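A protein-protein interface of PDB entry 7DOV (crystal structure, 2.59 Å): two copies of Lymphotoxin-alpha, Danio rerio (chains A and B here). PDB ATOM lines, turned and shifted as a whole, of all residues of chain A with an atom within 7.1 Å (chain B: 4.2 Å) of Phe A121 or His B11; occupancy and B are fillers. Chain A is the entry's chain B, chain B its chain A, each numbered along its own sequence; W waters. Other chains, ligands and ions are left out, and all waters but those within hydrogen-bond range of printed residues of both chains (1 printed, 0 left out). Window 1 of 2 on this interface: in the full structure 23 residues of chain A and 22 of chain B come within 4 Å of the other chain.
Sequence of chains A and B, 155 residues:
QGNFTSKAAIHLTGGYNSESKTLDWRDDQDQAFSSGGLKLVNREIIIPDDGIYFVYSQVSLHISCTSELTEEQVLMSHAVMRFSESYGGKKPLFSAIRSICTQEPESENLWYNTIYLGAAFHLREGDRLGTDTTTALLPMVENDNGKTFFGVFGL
Position printed for both chains: 56.
Of the 14 pairs that touch across the chains among the printed residues, none has its exchanged pair printed and touching as well.
Water W1 lies within hydrogen-bond range of the backbone carbonyl oxygen (O) of Gln B31 (2.5 Å) and the backbone NH (N) of His A122 (3.0 Å).
Of the printed residues of chain B, Leu A93 touches Gln B31 (3.4 Å).
Of the printed residues of chain B, Phe A94 touches Phe B149.
Of the printed residues of chain B, Ala A119 touches His B11 and Tyr B56.
Phe A121 touches just these residues of chain B: His B11 (3.7 Å), Gln B31 (3.8 Å) and Phe B33 (3.8 Å).
Of the printed residues of chain B, His A122 touches Phe B33.
Leu A155 touches none of the printed residues of chain B.
Ile B10 touches none of the printed residues of chain A.
His B11 touches just these residues of chain A: Ala A119, Ala A120 and Phe A121.
Printed residues of chain A within 4 Å of Phe B149: Phe A94 (3.8 Å).
The nearest residue of chain A that does not touch His B11 is Leu A93 (4.9 Å).
The nearest printed residue of chain B that does not touch Arg A82 is Ala B32 (8.3 Å).
Of the 9 printed residues of chain B, 5 touch a printed residue of chain A.
Hydrophobic or aromatic side chains of chain B within 4 Å of the printed part of chain A: His B11, Phe B33, Tyr B56 and Phe B149.
Along chain B the printed residues that touch a printed residue of chain A span positions 11 to 149.
Of the 19 printed residues of chain A, 9 touch a printed residue of chain B.
Among the printed residues, no Asp or Glu carboxylate lies within 4 Å of a Lys or Arg side-chain nitrogen of the other chain.
Ile A52 touches Phe B33 (CG2 to CZ, 3.8 Å).
CG of Gln B31 touches CD2 of Leu A93 (3.4 Å).
Phe A94 touches Phe B149 (CD2 to CZ, 3.8 Å).
O of Gly A118 touches CD1 of Tyr B56, 3.9 Å away.
Ala A119 touches His B11.
Ala A119 touches Tyr B56.
Ala A120 touches His B11 (O to CB, 3.5 Å).
Ala A120 touches Phe B33 (O to CE1, 3.6 Å).
Gln B31 touches Phe A121 (CB to CD1, 3.8 Å).
N of His A122 touches CE1 of Phe B33 (3.9 Å).
The guanidinium group (NH1) of Arg A82 is in hydrogen-bond range of the side-chain amide oxygen (OE1) of Gln B31 (3.1 Å).
OH of Tyr B56 sits at hydrogen-bond distance from N of Ala A120.
A ring nitrogen (ND1) of His B11 is in hydrogen-bond range of the side-chain hydroxyl of Tyr B56, at 2.9 Å.
N of Leu A93 sits at hydrogen-bond distance from O of Val A80 (2.7 Å).
The backbone NH (N) of Leu A155 sits at hydrogen-bond distance from the backbone carbonyl oxygen (O) of Ile A52 (2.9 Å).
O of Tyr A53 is in hydrogen-bond range of N of Phe A121.
N of Val A55 lies within hydrogen-bond range of O of Ala A119 (2.7 Å).
The backbone NH of His B11 is in hydrogen-bond range of the backbone carbonyl oxygen of Phe B33.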
ATOM      1  N   GLY A  51     -24.756 -33.508   0.117  1.00  0.00           N
ATOM      2  CA  GLY A  51     -24.458 -34.084  -1.195  1.00  0.00           C
ATOM      3  C   GLY A  51     -23.222 -33.507  -1.814  1.00  0.00           C
ATOM      4  O   GLY A  51     -22.590 -32.685  -1.193  1.00  0.00           O
ATOM      5  N   ILE A  52     -22.915 -33.953  -3.020  1.00  0.00           N
ATOM      6  CA  ILE A  52     -21.689 -33.468  -3.698  1.00  0.00           C
ATOM      7  C   ILE A  52     -22.026 -32.337  -4.658  1.00  0.00           C
ATOM      8  O   ILE A  52     -22.929 -32.454  -5.412  1.00  0.00           O
ATOM      9  CB  ILE A  52     -20.893 -34.607  -4.344  1.00  0.00           C
ATOM     10  CG1 ILE A  52     -20.482 -35.618  -3.286  1.00  0.00           C
ATOM     11  CG2 ILE A  52     -19.682 -34.058  -5.077  1.00  0.00           C
ATOM     12  CD1 ILE A  52     -20.464 -37.011  -3.784  1.00  0.00           C
ATOM     13  N   TYR A  53     -21.269 -31.267  -4.583  1.00  0.00           N
ATOM     14  CA  TYR A  53     -21.530 -30.115  -5.461  1.00  0.00           C
ATOM     15  C   TYR A  53     -20.249 -29.641  -6.139  1.00  0.00           C
ATOM     16  O   TYR A  53     -19.206 -29.644  -5.552  1.00  0.00           O
ATOM     17  CB  TYR A  53     -22.107 -28.961  -4.645  1.00  0.00           C
ATOM     18  CG  TYR A  53     -23.438 -29.208  -3.993  1.00  0.00           C
ATOM     19  CD1 TYR A  53     -23.528 -29.845  -2.772  1.00  0.00           C
ATOM     20  CD2 TYR A  53     -24.599 -28.742  -4.570  1.00  0.00           C
ATOM     21  CE1 TYR A  53     -24.749 -30.074  -2.179  1.00  0.00           C
ATOM     22  CE2 TYR A  53     -25.825 -28.939  -3.980  1.00  0.00           C
ATOM     23  CZ  TYR A  53     -25.900 -29.610  -2.781  1.00  0.00           C
ATOM     24  OH  TYR A  53     -27.110 -29.801  -2.207  1.00  0.00           O
ATOM     25  N   PHE A  54     -20.391 -29.251  -7.392  1.00  0.00           N
ATOM     26  CA  PHE A  54     -19.285 -28.612  -8.121  1.00  0.00           C
ATOM     27  C   PHE A  54     -19.397 -27.122  -7.834  1.00  0.00           C
ATOM     28  O   PHE A  54     -20.436 -26.598  -7.982  1.00  0.00           O
ATOM     29  CB  PHE A  54     -19.331 -28.904  -9.615  1.00  0.00           C
ATOM     30  CG  PHE A  54     -18.161 -28.332 -10.364  1.00  0.00           C
ATOM     31  CD1 PHE A  54     -16.960 -28.999 -10.405  1.00  0.00           C
ATOM     32  CD2 PHE A  54     -18.251 -27.115 -11.004  1.00  0.00           C
ATOM     33  CE1 PHE A  54     -15.882 -28.483 -11.087  1.00  0.00           C
ATOM     34  CE2 PHE A  54     -17.172 -26.599 -11.680  1.00  0.00           C
ATOM     35  CZ  PHE A  54     -15.994 -27.281 -11.715  1.00  0.00           C
ATOM     36  N   VAL A  55     -18.307 -26.507  -7.418  1.00  0.00           N
ATOM     37  CA  VAL A  55     -18.268 -25.068  -7.065  1.00  0.00           C
ATOM     38  C   VAL A  55     -17.273 -24.398  -8.001  1.00  0.00           C
ATOM     39  O   VAL A  55     -16.270 -24.940  -8.216  1.00  0.00           O
ATOM     40  CB  VAL A  55     -17.856 -24.921  -5.591  1.00  0.00           C
ATOM     41  CG1 VAL A  55     -17.738 -23.491  -5.119  1.00  0.00           C
ATOM     42  CG2 VAL A  55     -18.735 -25.739  -4.683  1.00  0.00           C
ATOM     43  N   TYR A  56     -17.595 -23.223  -8.500  1.00  0.00           N
ATOM     44  CA  TYR A  56     -16.708 -22.472  -9.415  1.00  0.00           C
ATOM     45  C   TYR A  56     -16.863 -20.959  -9.221  1.00  0.00           C
ATOM     46  O   TYR A  56     -17.866 -20.511  -8.753  1.00  0.00           O
ATOM     47  CB  TYR A  56     -16.921 -22.919 -10.861  1.00  0.00           C
ATOM     48  CG  TYR A  56     -18.257 -22.573 -11.450  1.00  0.00           C
ATOM     49  CD1 TYR A  56     -18.462 -21.351 -12.035  1.00  0.00           C
ATOM     50  CD2 TYR A  56     -19.310 -23.459 -11.412  1.00  0.00           C
ATOM     51  CE1 TYR A  56     -19.680 -21.008 -12.564  1.00  0.00           C
ATOM     52  CE2 TYR A  56     -20.536 -23.137 -11.948  1.00  0.00           C
ATOM     53  CZ  TYR A  56     -20.722 -21.901 -12.521  1.00  0.00           C
ATOM     54  OH  TYR A  56     -21.905 -21.538 -13.058  1.00  0.00           O
ATOM     55  N   VAL A  80     -13.033 -19.355  -2.118  1.00  0.00           N
ATOM     56  CA  VAL A  80     -14.433 -19.715  -1.783  1.00  0.00           C
ATOM     57  C   VAL A  80     -14.354 -20.281  -0.373  1.00  0.00           C
ATOM     58  O   VAL A  80     -13.618 -21.204  -0.165  1.00  0.00           O
ATOM     59  CB  VAL A  80     -15.082 -20.679  -2.789  1.00  0.00           C
ATOM     60  CG1 VAL A  80     -16.447 -21.120  -2.332  1.00  0.00           C
ATOM     61  CG2 VAL A  80     -15.195 -20.058  -4.151  1.00  0.00           C
ATOM     62  N   ARG A  82     -16.231 -21.831   3.143  1.00  0.00           N
ATOM     63  CA  ARG A  82     -17.419 -22.621   3.499  1.00  0.00           C
ATOM     64  C   ARG A  82     -17.760 -22.384   4.962  1.00  0.00           C
ATOM     65  O   ARG A  82     -16.885 -22.430   5.781  1.00  0.00           O
ATOM     66  CB  ARG A  82     -17.197 -24.096   3.192  1.00  0.00           C
ATOM     67  CG  ARG A  82     -18.263 -25.025   3.735  1.00  0.00           C
ATOM     68  CD  ARG A  82     -17.708 -26.409   3.653  1.00  0.00           C
ATOM     69  NE  ARG A  82     -18.693 -27.352   4.092  1.00  0.00           N
ATOM     70  CZ  ARG A  82     -18.440 -28.446   4.765  1.00  0.00           C
ATOM     71  NH1 ARG A  82     -17.204 -28.755   5.071  1.00  0.00           N
ATOM     72  NH2 ARG A  82     -19.422 -29.238   5.117  1.00  0.00           N
ATOM     73  N   PRO A  92     -11.527 -22.471   3.878  1.00  0.00           N
ATOM     74  CA  PRO A  92     -11.154 -22.174   2.266  1.00  0.00           C
ATOM     75  C   PRO A  92     -11.568 -23.506   1.647  1.00  0.00           C
ATOM     76  O   PRO A  92     -11.163 -24.493   2.130  1.00  0.00           O
ATOM     77  CB  PRO A  92      -9.661 -21.919   2.240  1.00  0.00           C
ATOM     78  CG  PRO A  92      -9.352 -21.546   3.649  1.00  0.00           C
ATOM     79  CD  PRO A  92     -10.212 -22.444   4.498  1.00  0.00           C
ATOM     80  N   LEU A  93     -12.480 -23.483   0.685  1.00  0.00           N
ATOM     81  CA  LEU A  93     -12.800 -24.732  -0.036  1.00  0.00           C
ATOM     82  C   LEU A  93     -11.633 -24.898  -0.996  1.00  0.00           C
ATOM     83  O   LEU A  93     -11.176 -25.989  -1.153  1.00  0.00           O
ATOM     84  CB  LEU A  93     -14.104 -24.560  -0.813  1.00  0.00           C
ATOM     85  CG  LEU A  93     -15.356 -25.096  -0.143  1.00  0.00           C
ATOM     86  CD1 LEU A  93     -16.502 -25.195  -1.129  1.00  0.00           C
ATOM     87  CD2 LEU A  93     -15.082 -26.417   0.515  1.00  0.00           C
ATOM     88  N   PHE A  94     -11.176 -23.782  -1.543  1.00  0.00           N
ATOM     89  CA  PHE A  94     -10.035 -23.647  -2.478  1.00  0.00           C
ATOM     90  C   PHE A  94      -9.747 -22.163  -2.687  1.00  0.00           C
ATOM     91  O   PHE A  94     -10.558 -21.364  -2.348  1.00  0.00           O
ATOM     92  CB  PHE A  94     -10.241 -24.419  -3.791  1.00  0.00           C
ATOM     93  CG  PHE A  94     -11.472 -24.147  -4.614  1.00  0.00           C
ATOM     94  CD1 PHE A  94     -12.478 -23.323  -4.173  1.00  0.00           C
ATOM     95  CD2 PHE A  94     -11.626 -24.737  -5.841  1.00  0.00           C
ATOM     96  CE1 PHE A  94     -13.588 -23.088  -4.949  1.00  0.00           C
ATOM     97  CE2 PHE A  94     -12.746 -24.516  -6.609  1.00  0.00           C
ATOM     98  CZ  PHE A  94     -13.727 -23.689  -6.161  1.00  0.00           C
ATOM     99  N   GLY A 118     -12.567 -24.110 -10.012  1.00  0.00           N
ATOM    100  CA  GLY A 118     -13.772 -24.952 -10.014  1.00  0.00           C
ATOM    101  C   GLY A 118     -13.495 -26.335  -9.481  1.00  0.00           C
ATOM    102  O   GLY A 118     -12.609 -26.929 -10.004  1.00  0.00           O
ATOM    103  N   ALA A 119     -14.237 -26.827  -8.497  1.00  0.00           N
ATOM    104  CA  ALA A 119     -13.974 -28.183  -7.978  1.00  0.00           C
ATOM    105  C   ALA A 119     -15.222 -28.785  -7.326  1.00  0.00           C
ATOM    106  O   ALA A 119     -16.139 -28.075  -7.042  1.00  0.00           O
ATOM    107  CB  ALA A 119     -12.805 -28.154  -7.035  1.00  0.00           C
ATOM    108  N   ALA A 120     -15.218 -30.093  -7.130  1.00  0.00           N
ATOM    109  CA  ALA A 120     -16.329 -30.789  -6.459  1.00  0.00           C
ATOM    110  C   ALA A 120     -15.999 -30.935  -4.976  1.00  0.00           C
ATOM    111  O   ALA A 120     -14.857 -31.156  -4.655  1.00  0.00           O
ATOM    112  CB  ALA A 120     -16.630 -32.098  -7.122  1.00  0.00           C
ATOM    113  N   PHE A 121     -16.990 -30.716  -4.127  1.00  0.00           N
ATOM    114  CA  PHE A 121     -16.817 -30.793  -2.664  1.00  0.00           C
ATOM    115  C   PHE A 121     -18.038 -31.442  -2.042  1.00  0.00           C
ATOM    116  O   PHE A 121     -19.103 -31.313  -2.567  1.00  0.00           O
ATOM    117  CB  PHE A 121     -16.686 -29.393  -2.063  1.00  0.00           C
ATOM    118  CG  PHE A 121     -15.469 -28.645  -2.522  1.00  0.00           C
ATOM    119  CD1 PHE A 121     -14.237 -28.875  -1.945  1.00  0.00           C
ATOM    120  CD2 PHE A 121     -15.544 -27.773  -3.580  1.00  0.00           C
ATOM    121  CE1 PHE A 121     -13.117 -28.218  -2.404  1.00  0.00           C
ATOM    122  CE2 PHE A 121     -14.422 -27.114  -4.029  1.00  0.00           C
ATOM    123  CZ  PHE A 121     -13.213 -27.336  -3.437  1.00  0.00           C
ATOM    124  N   HIS A 122     -17.831 -32.120  -0.927  1.00  0.00           N
ATOM    125  CA  HIS A 122     -18.948 -32.710  -0.160  1.00  0.00           C
ATOM    126  C   HIS A 122     -19.471 -31.656   0.807  1.00  0.00           C
ATOM    127  O   HIS A 122     -18.706 -31.208   1.604  1.00  0.00           O
ATOM    128  CB  HIS A 122     -18.532 -33.979   0.567  1.00  0.00           C
ATOM    129  CG  HIS A 122     -19.718 -34.558   1.229  1.00  0.00           C
ATOM    130  ND1 HIS A 122     -20.052 -34.249   2.493  1.00  0.00           N
ATOM    131  CD2 HIS A 122     -20.714 -35.316   0.757  1.00  0.00           C
ATOM    132  CE1 HIS A 122     -21.170 -34.831   2.793  1.00  0.00           C
ATOM    133  NE2 HIS A 122     -21.585 -35.485   1.759  1.00  0.00           N
ATOM    134  N   LEU A 123     -20.743 -31.281   0.694  1.00  0.00           N
ATOM    135  CA  LEU A 123     -21.335 -30.212   1.540  1.00  0.00           C
ATOM    136  C   LEU A 123     -22.559 -30.713   2.299  1.00  0.00           C
ATOM    137  O   LEU A 123     -23.103 -31.720   1.929  1.00  0.00           O
ATOM    138  CB  LEU A 123     -21.677 -29.010   0.664  1.00  0.00           C
ATOM    139  CG  LEU A 123     -20.492 -28.408  -0.069  1.00  0.00           C
ATOM    140  CD1 LEU A 123     -20.936 -27.384  -1.079  1.00  0.00           C
ATOM    141  CD2 LEU A 123     -19.524 -27.806   0.918  1.00  0.00           C
ATOM    142  N   LEU A 129     -21.806 -20.685   1.172  1.00  0.00           N
ATOM    143  CA  LEU A 129     -20.543 -20.446   0.441  1.00  0.00           C
ATOM    144  C   LEU A 129     -20.382 -18.958   0.147  1.00  0.00           C
ATOM    145  O   LEU A 129     -21.307 -18.333  -0.248  1.00  0.00           O
ATOM    146  CB  LEU A 129     -20.505 -21.289  -0.830  1.00  0.00           C
ATOM    147  CG  LEU A 129     -20.686 -22.789  -0.669  1.00  0.00           C
ATOM    148  CD1 LEU A 129     -20.510 -23.468  -1.986  1.00  0.00           C
ATOM    149  CD2 LEU A 129     -19.748 -23.392   0.340  1.00  0.00           C
ATOM    150  N   LEU A 155     -24.031 -32.561  -8.051  1.00  0.00           N
ATOM    151  CA  LEU A 155     -23.604 -33.665  -8.926  1.00  0.00           C
ATOM    152  C   LEU A 155     -24.650 -34.771  -8.871  1.00  0.00           C
ATOM    153  O   LEU A 155     -24.694 -35.520  -9.794  1.00  0.00           O
ATOM    154  CB  LEU A 155     -22.250 -34.173  -8.443  1.00  0.00           C
ATOM    155  CG  LEU A 155     -21.023 -33.568  -9.113  1.00  0.00           C
ATOM    156  CD1 LEU A 155     -21.238 -32.132  -9.498  1.00  0.00           C
ATOM    157  CD2 LEU A 155     -19.836 -33.676  -8.202  1.00  0.00           C
ATOM    158  OXT LEU A 155     -25.394 -34.841  -7.892  1.00  0.00           O
ATOM    159  N   ILE B  10     -14.254 -37.539  -6.331  1.00  0.00           N
ATOM    160  CA  ILE B  10     -13.073 -37.548  -5.449  1.00  0.00           C
ATOM    161  C   ILE B  10     -12.405 -36.177  -5.541  1.00  0.00           C
ATOM    162  O   ILE B  10     -12.374 -35.610  -6.591  1.00  0.00           O
ATOM    163  CB  ILE B  10     -12.157 -38.732  -5.831  1.00  0.00           C
ATOM    164  CG1 ILE B  10     -10.997 -38.900  -4.851  1.00  0.00           C
ATOM    165  CG2 ILE B  10     -11.689 -38.652  -7.269  1.00  0.00           C
ATOM    166  CD1 ILE B  10     -10.161 -40.112  -5.085  1.00  0.00           C
ATOM    167  N   HIS B  11     -11.943 -35.649  -4.426  1.00  0.00           N
ATOM    168  CA  HIS B  11     -11.192 -34.379  -4.440  1.00  0.00           C
ATOM    169  C   HIS B  11      -9.960 -34.587  -3.570  1.00  0.00           C
ATOM    170  O   HIS B  11     -10.117 -35.005  -2.463  1.00  0.00           O
ATOM    171  CB  HIS B  11     -12.065 -33.211  -4.011  1.00  0.00           C
ATOM    172  CG  HIS B  11     -11.323 -31.925  -3.940  1.00  0.00           C
ATOM    173  ND1 HIS B  11     -11.065 -31.179  -5.027  1.00  0.00           N
ATOM    174  CD2 HIS B  11     -10.745 -31.290  -2.917  1.00  0.00           C
ATOM    175  CE1 HIS B  11     -10.403 -30.126  -4.679  1.00  0.00           C
ATOM    176  NE2 HIS B  11     -10.203 -30.174  -3.410  1.00  0.00           N
ATOM    177  N   LEU B  12      -8.781 -34.326  -4.121  1.00  0.00           N
ATOM    178  CA  LEU B  12      -7.503 -34.515  -3.413  1.00  0.00           C
ATOM    179  C   LEU B  12      -6.822 -33.168  -3.243  1.00  0.00           C
ATOM    180  O   LEU B  12      -6.980 -32.312  -4.082  1.00  0.00           O
ATOM    181  CB  LEU B  12      -6.595 -35.418  -4.246  1.00  0.00           C
ATOM    182  CG  LEU B  12      -7.084 -36.817  -4.601  1.00  0.00           C
ATOM    183  CD1 LEU B  12      -6.018 -37.549  -5.368  1.00  0.00           C
ATOM    184  CD2 LEU B  12      -7.462 -37.626  -3.384  1.00  0.00           C
ATOM    185  N   GLN B  31     -10.570 -30.287   2.612  1.00  0.00           N
ATOM    186  CA  GLN B  31     -11.892 -30.603   2.019  1.00  0.00           C
ATOM    187  C   GLN B  31     -11.829 -31.784   1.054  1.00  0.00           C
ATOM    188  O   GLN B  31     -12.658 -31.857   0.176  1.00  0.00           O
ATOM    189  CB  GLN B  31     -12.459 -29.369   1.332  1.00  0.00           C
ATOM    190  CG  GLN B  31     -12.853 -28.249   2.279  1.00  0.00           C
ATOM    191  CD  GLN B  31     -13.916 -28.562   3.301  1.00  0.00           C
ATOM    192  OE1 GLN B  31     -14.985 -29.068   2.998  1.00  0.00           O
ATOM    193  NE2 GLN B  31     -13.629 -28.219   4.537  1.00  0.00           N
ATOM    194  N   ALA B  32     -10.926 -32.720   1.304  1.00  0.00           N
ATOM    195  CA  ALA B  32     -10.738 -33.908   0.450  1.00  0.00           C
ATOM    196  C   ALA B  32     -11.786 -34.959   0.772  1.00  0.00           C
ATOM    197  O   ALA B  32     -12.172 -35.046   1.902  1.00  0.00           O
ATOM    198  CB  ALA B  32      -9.360 -34.461   0.667  1.00  0.00           C
ATOM    199  N   PHE B  33     -12.179 -35.745  -0.216  1.00  0.00           N
ATOM    200  CA  PHE B  33     -13.178 -36.814  -0.009  1.00  0.00           C
ATOM    201  C   PHE B  33     -13.118 -37.793  -1.173  1.00  0.00           C
ATOM    202  O   PHE B  33     -12.601 -37.469  -2.201  1.00  0.00           O
ATOM    203  CB  PHE B  33     -14.578 -36.219   0.125  1.00  0.00           C
ATOM    204  CG  PHE B  33     -15.203 -35.832  -1.177  1.00  0.00           C
ATOM    205  CD1 PHE B  33     -14.866 -34.648  -1.790  1.00  0.00           C
ATOM    206  CD2 PHE B  33     -16.091 -36.677  -1.804  1.00  0.00           C
ATOM    207  CE1 PHE B  33     -15.419 -34.308  -3.005  1.00  0.00           C
ATOM    208  CE2 PHE B  33     -16.652 -36.328  -3.012  1.00  0.00           C
ATOM    209  CZ  PHE B  33     -16.312 -35.144  -3.610  1.00  0.00           C
ATOM    210  N   TYR B  56     -10.204 -32.403 -13.205  1.00  0.00           N
ATOM    211  CA  TYR B  56      -9.679 -31.045 -12.965  1.00  0.00           C
ATOM    212  C   TYR B  56      -8.438 -31.125 -12.079  1.00  0.00           C
ATOM    213  O   TYR B  56      -8.275 -32.076 -11.403  1.00  0.00           O
ATOM    214  CB  TYR B  56     -10.766 -30.150 -12.371  1.00  0.00           C
ATOM    215  CG  TYR B  56     -11.298 -30.599 -11.041  1.00  0.00           C
ATOM    216  CD1 TYR B  56     -10.630 -30.289  -9.878  1.00  0.00           C
ATOM    217  CD2 TYR B  56     -12.460 -31.337 -10.954  1.00  0.00           C
ATOM    218  CE1 TYR B  56     -11.088 -30.726  -8.662  1.00  0.00           C
ATOM    219  CE2 TYR B  56     -12.942 -31.767  -9.739  1.00  0.00           C
ATOM    220  CZ  TYR B  56     -12.251 -31.452  -8.590  1.00  0.00           C
ATOM    221  OH  TYR B  56     -12.677 -31.864  -7.385  1.00  0.00           O
ATOM    222  N   PHE B 149      -4.748 -28.931  -5.971  1.00  0.00           N
ATOM    223  CA  PHE B 149      -5.688 -30.065  -5.835  1.00  0.00           C
ATOM    224  C   PHE B 149      -5.862 -30.806  -7.163  1.00  0.00           C
ATOM    225  O   PHE B 149      -5.489 -30.323  -8.209  1.00  0.00           O
ATOM    226  CB  PHE B 149      -7.021 -29.571  -5.268  1.00  0.00           C
ATOM    227  CG  PHE B 149      -7.637 -28.469  -6.075  1.00  0.00           C
ATOM    228  CD1 PHE B 149      -8.370 -28.744  -7.208  1.00  0.00           C
ATOM    229  CD2 PHE B 149      -7.433 -27.156  -5.735  1.00  0.00           C
ATOM    230  CE1 PHE B 149      -8.885 -27.732  -7.981  1.00  0.00           C
ATOM    231  CE2 PHE B 149      -7.970 -26.146  -6.501  1.00  0.00           C
ATOM    232  CZ  PHE B 149      -8.705 -26.438  -7.614  1.00  0.00           C
ATOM    233  N   PHE B 150      -6.489 -31.965  -7.055  1.00  0.00           N
ATOM    234  CA  PHE B 150      -6.733 -32.879  -8.180  1.00  0.00           C
ATOM    235  C   PHE B 150      -8.082 -33.561  -7.933  1.00  0.00           C
ATOM    236  O   PHE B 150      -8.322 -34.002  -6.875  1.00  0.00           O
ATOM    237  CB  PHE B 150      -5.512 -33.792  -8.257  1.00  0.00           C
ATOM    238  CG  PHE B 150      -5.462 -34.817  -9.350  1.00  0.00           C
ATOM    239  CD1 PHE B 150      -6.061 -34.587 -10.568  1.00  0.00           C
ATOM    240  CD2 PHE B 150      -4.821 -36.020  -9.143  1.00  0.00           C
ATOM    241  CE1 PHE B 150      -6.002 -35.538 -11.563  1.00  0.00           C
ATOM    242  CE2 PHE B 150      -4.757 -36.967 -10.143  1.00  0.00           C
ATOM    243  CZ  PHE B 150      -5.352 -36.723 -11.347  1.00  0.00           C
HETATM  244  O   HOH W   1     -15.194 -31.939   0.398  1.00  0.00           O
